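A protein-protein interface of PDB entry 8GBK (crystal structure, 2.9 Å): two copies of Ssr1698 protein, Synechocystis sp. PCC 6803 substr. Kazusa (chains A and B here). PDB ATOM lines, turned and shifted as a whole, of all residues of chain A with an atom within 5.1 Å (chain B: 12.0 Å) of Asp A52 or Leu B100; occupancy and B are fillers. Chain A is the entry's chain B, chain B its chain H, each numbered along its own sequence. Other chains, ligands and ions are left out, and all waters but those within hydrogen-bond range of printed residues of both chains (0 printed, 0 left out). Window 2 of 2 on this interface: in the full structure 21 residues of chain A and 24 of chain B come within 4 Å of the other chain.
N of Gln A44 is in hydrogen-bond range of O of Asp A52, at 2.8 Å.
The backbone carbonyl oxygen (O) of Ala A45 lies within hydrogen-bond range of the backbone NH (N) of Asp A52.
The guanidinium group (NH1) of Arg A65 lies within salt-bridge range of the side-chain carboxylate (OD2) of Asp A47.
O of Gly A50 lies within hydrogen-bond range of NH2 of Arg A65 (3.3 Å).
NH1 of Arg A65 is in salt-bridge range of OD1 of Asp A52 (2.7 Å).
O of Ile A64 is in hydrogen-bond range of N of Leu A53 (3.0 Å).
No position is printed for both chains.
Of the 10 pairs that touch across the chains among the printed residues, none has its exchanged pair printed and touching as well.
Of the 6 printed residues of chain B, 5 touch a printed residue of chain A.
The backbone NH of Glu B98 sits at hydrogen-bond distance from the backbone carbonyl oxygen of Arg A65 (3.1 Å).
The backbone NH (N) of Leu B100 is in hydrogen-bond range of the backbone carbonyl oxygen (O) of Thr A63.
Among the printed residues, merely in contact across the chains: Asp A52 with Leu B100 (3.5 Å), Thr A63 with Asn B99 (3.9 Å), Ile A64 with Glu B98 (3.7 Å), Ile A64 with Asn B99 (3.8 Å), Ile A64 with Leu B100 (3.9 Å), Arg A65 with Ser B96 (3.9 Å), Arg A65 with Ala B97 (3.9 Å) and Arg A65 with Leu B100 (3.8 Å).
Leu B100 touches just these residues of chain A: Asp A52 (3.5 Å), Thr A63 (3.1 Å), Ile A64 (3.9 Å) and Arg A65 (3.8 Å).
Met A43 touches none of the printed residues of chain B.
No residue of chain B comes within 4 Å of Gln A44.
No residue of chain B comes within 4 Å of Ala A45.
No residue of chain B comes within 4 Å of Ile A46.
No residue of chain B comes within 4 Å of Asp A47.
No residue of chain B comes within 4 Å of Gly A50.
No residue of chain B comes within 4 Å of Leu A53.
Val A54 touches none of the printed residues of chain B.
Of chain B, only Asn B99 (3.9 Å) and Leu B100 (3.1 Å) come within 4 Å of Thr A63.
Ile A64 touches just these residues of chain B: Glu B98 (3.7 Å), Asn B99 (3.8 Å) and Leu B100 (3.9 Å).
Of chain B, only Ser B96 (3.9 Å), Ala B97 (3.9 Å), Glu B98 (3.1 Å) and Leu B100 (3.8 Å) come within 4 Å of Arg A65.
Printed residues of chain A within 4 Å of Ala B97: Arg A65.
Of the printed residues of chain A, Ser B96 touches Arg A65.
Of the printed residues of chain A, Asn B99 touches Thr A63 (3.9 Å) and Ile A64 (3.8 Å).
Of the printed residues of chain A, Glu B98 touches Ile A64 and Arg A65.
The nearest residue of chain B that does not touch Asp A52 is Asn B99 (7.6 Å).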
ATOM      1  N   GLN A  42      20.838  23.895   3.847  1.00  0.00           N
ATOM      2  CA  GLN A  42      21.668  23.413   4.974  1.00  0.00           C
ATOM      3  C   GLN A  42      20.829  22.885   6.134  1.00  0.00           C
ATOM      4  O   GLN A  42      19.749  23.388   6.309  1.00  0.00           O
ATOM      5  CB  GLN A  42      22.442  24.612   5.503  1.00  0.00           C
ATOM      6  CG  GLN A  42      23.269  25.343   4.457  1.00  0.00           C
ATOM      7  CD  GLN A  42      23.917  26.574   5.035  1.00  0.00           C
ATOM      8  OE1 GLN A  42      23.259  27.430   5.618  1.00  0.00           O
ATOM      9  NE2 GLN A  42      25.226  26.672   4.884  1.00  0.00           N
ATOM     10  N   MET A  43      21.338  21.929   6.910  1.00  0.00           N
ATOM     11  CA  MET A  43      20.641  21.436   8.094  1.00  0.00           C
ATOM     12  C   MET A  43      21.352  22.024   9.307  1.00  0.00           C
ATOM     13  O   MET A  43      22.394  21.521   9.734  1.00  0.00           O
ATOM     14  CB  MET A  43      20.618  19.912   8.125  1.00  0.00           C
ATOM     15  CG  MET A  43      19.654  19.339   9.151  1.00  0.00           C
ATOM     16  SD  MET A  43      19.494  17.546   9.039  1.00  0.00           S
ATOM     17  CE  MET A  43      18.584  17.382   7.507  1.00  0.00           C
ATOM     18  N   GLN A  44      20.778  23.090   9.865  1.00  0.00           N
ATOM     19  CA  GLN A  44      21.415  23.774  10.985  1.00  0.00           C
ATOM     20  C   GLN A  44      21.338  22.940  12.257  1.00  0.00           C
ATOM     21  O   GLN A  44      22.333  22.790  12.973  1.00  0.00           O
ATOM     22  CB  GLN A  44      20.771  25.145  11.195  1.00  0.00           C
ATOM     23  CG  GLN A  44      21.210  25.856  12.465  1.00  0.00           C
ATOM     24  CD  GLN A  44      20.364  27.078  12.776  1.00  0.00           C
ATOM     25  OE1 GLN A  44      19.686  27.134  13.800  1.00  0.00           O
ATOM     26  NE2 GLN A  44      20.408  28.068  11.890  1.00  0.00           N
ATOM     27  N   ALA A  45      20.166  22.383  12.551  1.00  0.00           N
ATOM     28  CA  ALA A  45      19.994  21.608  13.770  1.00  0.00           C
ATOM     29  C   ALA A  45      18.804  20.681  13.601  1.00  0.00           C
ATOM     30  O   ALA A  45      17.891  20.957  12.818  1.00  0.00           O
ATOM     31  CB  ALA A  45      19.796  22.512  14.990  1.00  0.00           C
ATOM     32  N   ILE A  46      18.822  19.581  14.347  1.00  0.00           N
ATOM     33  CA  ILE A  46      17.740  18.608  14.342  1.00  0.00           C
ATOM     34  C   ILE A  46      17.324  18.336  15.779  1.00  0.00           C
ATOM     35  O   ILE A  46      18.165  18.295  16.682  1.00  0.00           O
ATOM     36  CB  ILE A  46      18.155  17.301  13.637  1.00  0.00           C
ATOM     37  CG1 ILE A  46      16.949  16.374  13.490  1.00  0.00           C
ATOM     38  CG2 ILE A  46      19.274  16.618  14.403  1.00  0.00           C
ATOM     39  CD1 ILE A  46      17.168  15.238  12.517  1.00  0.00           C
ATOM     40  N   ASP A  47      16.027  18.156  15.984  1.00  0.00           N
ATOM     41  CA  ASP A  47      15.440  17.948  17.298  1.00  0.00           C
ATOM     42  C   ASP A  47      14.426  16.824  17.213  1.00  0.00           C
ATOM     43  O   ASP A  47      13.967  16.472  16.119  1.00  0.00           O
ATOM     44  CB  ASP A  47      14.769  19.221  17.834  1.00  0.00           C
ATOM     45  CG  ASP A  47      15.746  20.368  18.006  1.00  0.00           C
ATOM     46  OD1 ASP A  47      16.737  20.201  18.748  1.00  0.00           O
ATOM     47  OD2 ASP A  47      15.524  21.440  17.403  1.00  0.00           O
ATOM     48  N   GLY A  50      11.541  18.401  15.275  1.00  0.00           N
ATOM     49  CA  GLY A  50      11.766  18.744  13.889  1.00  0.00           C
ATOM     50  C   GLY A  50      13.204  19.140  13.657  1.00  0.00           C
ATOM     51  O   GLY A  50      14.056  19.020  14.539  1.00  0.00           O
ATOM     52  N   MET A  51      13.463  19.619  12.444  1.00  0.00           N
ATOM     53  CA  MET A  51      14.788  20.059  12.045  1.00  0.00           C
ATOM     54  C   MET A  51      14.684  21.465  11.478  1.00  0.00           C
ATOM     55  O   MET A  51      13.630  21.875  10.985  1.00  0.00           O
ATOM     56  CB  MET A  51      15.409  19.130  11.001  1.00  0.00           C
ATOM     57  CG  MET A  51      14.548  18.940   9.767  1.00  0.00           C
ATOM     58  SD  MET A  51      15.306  17.852   8.548  1.00  0.00           S
ATOM     59  CE  MET A  51      14.010  17.783   7.313  1.00  0.00           C
ATOM     60  N   ASP A  52      15.785  22.200  11.556  1.00  0.00           N
ATOM     61  CA  ASP A  52      15.855  23.569  11.065  1.00  0.00           C
ATOM     62  C   ASP A  52      16.759  23.607   9.840  1.00  0.00           C
ATOM     63  O   ASP A  52      17.932  23.226   9.921  1.00  0.00           O
ATOM     64  CB  ASP A  52      16.373  24.504  12.155  1.00  0.00           C
ATOM     65  CG  ASP A  52      15.623  24.341  13.462  1.00  0.00           C
ATOM     66  OD1 ASP A  52      15.778  23.283  14.108  1.00  0.00           O
ATOM     67  OD2 ASP A  52      14.878  25.267  13.842  1.00  0.00           O
ATOM     68  N   LEU A  53      16.191  23.992   8.705  1.00  0.00           N
ATOM     69  CA  LEU A  53      16.985  24.076   7.464  1.00  0.00           C
ATOM     70  C   LEU A  53      17.250  25.547   7.163  1.00  0.00           C
ATOM     71  O   LEU A  53      16.417  26.381   7.541  1.00  0.00           O
ATOM     72  CB  LEU A  53      16.233  23.413   6.312  1.00  0.00           C
ATOM     73  CG  LEU A  53      15.788  21.967   6.502  1.00  0.00           C
ATOM     74  CD1 LEU A  53      15.304  21.404   5.182  1.00  0.00           C
ATOM     75  CD2 LEU A  53      16.920  21.112   7.036  1.00  0.00           C
ATOM     76  N   VAL A  54      18.375  25.841   6.504  1.00  0.00           N
ATOM     77  CA  VAL A  54      18.740  27.247   6.152  1.00  0.00           C
ATOM     78  C   VAL A  54      19.019  27.306   4.645  1.00  0.00           C
ATOM     79  O   VAL A  54      19.909  26.564   4.179  1.00  0.00           O
ATOM     80  CB  VAL A  54      19.940  27.734   6.990  1.00  0.00           C
ATOM     81  CG1 VAL A  54      20.426  29.118   6.583  1.00  0.00           C
ATOM     82  CG2 VAL A  54      19.634  27.701   8.478  1.00  0.00           C
ATOM     83  N   THR A  63      15.435  30.918   7.140  1.00  0.00           N
ATOM     84  CA  THR A  63      15.385  30.148   8.412  1.00  0.00           C
ATOM     85  C   THR A  63      14.025  29.446   8.459  1.00  0.00           C
ATOM     86  O   THR A  63      13.018  30.134   8.724  1.00  0.00           O
ATOM     87  CB  THR A  63      15.672  31.057   9.613  1.00  0.00           C
ATOM     88  OG1 THR A  63      14.792  32.183   9.578  1.00  0.00           O
ATOM     89  CG2 THR A  63      17.105  31.538   9.650  1.00  0.00           C
ATOM     90  N   ILE A  64      13.995  28.136   8.199  1.00  0.00           N
ATOM     91  CA  ILE A  64      12.687  27.415   8.093  1.00  0.00           C
ATOM     92  C   ILE A  64      12.675  26.172   8.995  1.00  0.00           C
ATOM     93  O   ILE A  64      13.748  25.626   9.257  1.00  0.00           O
ATOM     94  CB  ILE A  64      12.346  27.061   6.632  1.00  0.00           C
ATOM     95  CG1 ILE A  64      13.378  26.137   5.984  1.00  0.00           C
ATOM     96  CG2 ILE A  64      12.122  28.317   5.807  1.00  0.00           C
ATOM     97  CD1 ILE A  64      12.772  25.106   5.069  1.00  0.00           C
ATOM     98  N   ARG A  65      11.492  25.760   9.462  1.00  0.00           N
ATOM     99  CA  ARG A  65      11.377  24.585  10.358  1.00  0.00           C
ATOM    100  C   ARG A  65      10.467  23.522   9.761  1.00  0.00           C
ATOM    101  O   ARG A  65       9.333  23.846   9.412  1.00  0.00           O
ATOM    102  CB  ARG A  65      10.787  24.974  11.705  1.00  0.00           C
ATOM    103  CG  ARG A  65      10.590  23.811  12.665  1.00  0.00           C
ATOM    104  CD  ARG A  65      11.889  23.451  13.348  1.00  0.00           C
ATOM    105  NE  ARG A  65      11.763  22.377  14.318  1.00  0.00           N
ATOM    106  CZ  ARG A  65      12.541  22.243  15.381  1.00  0.00           C
ATOM    107  NH1 ARG A  65      13.497  23.121  15.624  1.00  0.00           N
ATOM    108  NH2 ARG A  65      12.358  21.240  16.211  1.00  0.00           N
ATOM    109  N   THR B  36       2.899  28.166  -1.786  1.00  0.00           N
ATOM    110  CA  THR B  36       2.765  28.074  -0.318  1.00  0.00           C
ATOM    111  C   THR B  36       1.379  28.570   0.083  1.00  0.00           C
ATOM    112  O   THR B  36       0.630  27.804   0.710  1.00  0.00           O
ATOM    113  CB  THR B  36       3.911  28.851   0.340  1.00  0.00           C
ATOM    114  OG1 THR B  36       5.141  28.189   0.046  1.00  0.00           O
ATOM    115  CG2 THR B  36       3.766  29.008   1.838  1.00  0.00           C
ATOM    116  N   SER B  96       4.252  19.574   8.182  1.00  0.00           N
ATOM    117  CA  SER B  96       4.021  21.005   8.051  1.00  0.00           C
ATOM    118  C   SER B  96       5.337  21.757   7.892  1.00  0.00           C
ATOM    119  O   SER B  96       6.346  21.423   8.520  1.00  0.00           O
ATOM    120  CB  SER B  96       3.255  21.536   9.264  1.00  0.00           C
ATOM    121  OG  SER B  96       3.997  21.367  10.460  1.00  0.00           O
ATOM    122  N   ALA B  97       5.320  22.777   7.042  1.00  0.00           N
ATOM    123  CA  ALA B  97       6.453  23.669   6.845  1.00  0.00           C
ATOM    124  C   ALA B  97       6.125  25.026   7.451  1.00  0.00           C
ATOM    125  O   ALA B  97       5.093  25.624   7.124  1.00  0.00           O
ATOM    126  CB  ALA B  97       6.785  23.820   5.361  1.00  0.00           C
ATOM    127  N   GLU B  98       7.000  25.509   8.328  1.00  0.00           N
ATOM    128  CA  GLU B  98       6.777  26.791   8.983  1.00  0.00           C
ATOM    129  C   GLU B  98       8.008  27.681   8.864  1.00  0.00           C
ATOM    130  O   GLU B  98       8.937  27.367   8.113  1.00  0.00           O
ATOM    131  CB  GLU B  98       6.400  26.578  10.449  1.00  0.00           C
ATOM    132  CG  GLU B  98       5.142  25.750  10.642  1.00  0.00           C
ATOM    133  CD  GLU B  98       4.713  25.666  12.094  1.00  0.00           C
ATOM    134  OE1 GLU B  98       5.538  25.978  12.979  1.00  0.00           O
ATOM    135  OE2 GLU B  98       3.549  25.291  12.349  1.00  0.00           O
ATOM    136  N   ASN B  99       8.021  28.795   9.589  1.00  0.00           N
ATOM    137  CA  ASN B  99       9.135  29.729   9.567  1.00  0.00           C
ATOM    138  C   ASN B  99       9.673  29.941  10.976  1.00  0.00           C
ATOM    139  O   ASN B  99       8.971  29.743  11.971  1.00  0.00           O
ATOM    140  CB  ASN B  99       8.722  31.076   8.963  1.00  0.00           C
ATOM    141  CG  ASN B  99       8.751  31.063   7.452  1.00  0.00           C
ATOM    142  OD1 ASN B  99       9.807  31.212   6.841  1.00  0.00           O
ATOM    143  ND2 ASN B  99       7.589  30.882   6.839  1.00  0.00           N
ATOM    144  N   LEU B 100      10.935  30.349  11.045  1.00  0.00           N
ATOM    145  CA  LEU B 100      11.584  30.625  12.321  1.00  0.00           C
ATOM    146  C   LEU B 100      11.527  32.113  12.650  1.00  0.00           C
ATOM    147  O   LEU B 100      11.073  32.503  13.725  1.00  0.00           O
ATOM    148  CB  LEU B 100      13.037  30.145  12.298  1.00  0.00           C
ATOM    149  CG  LEU B 100      13.259  28.638  12.151  1.00  0.00           C
ATOM    150  CD1 LEU B 100      14.742  28.320  12.039  1.00  0.00           C
ATOM    151  CD2 LEU B 100      12.637  27.889  13.318  1.00  0.00           C
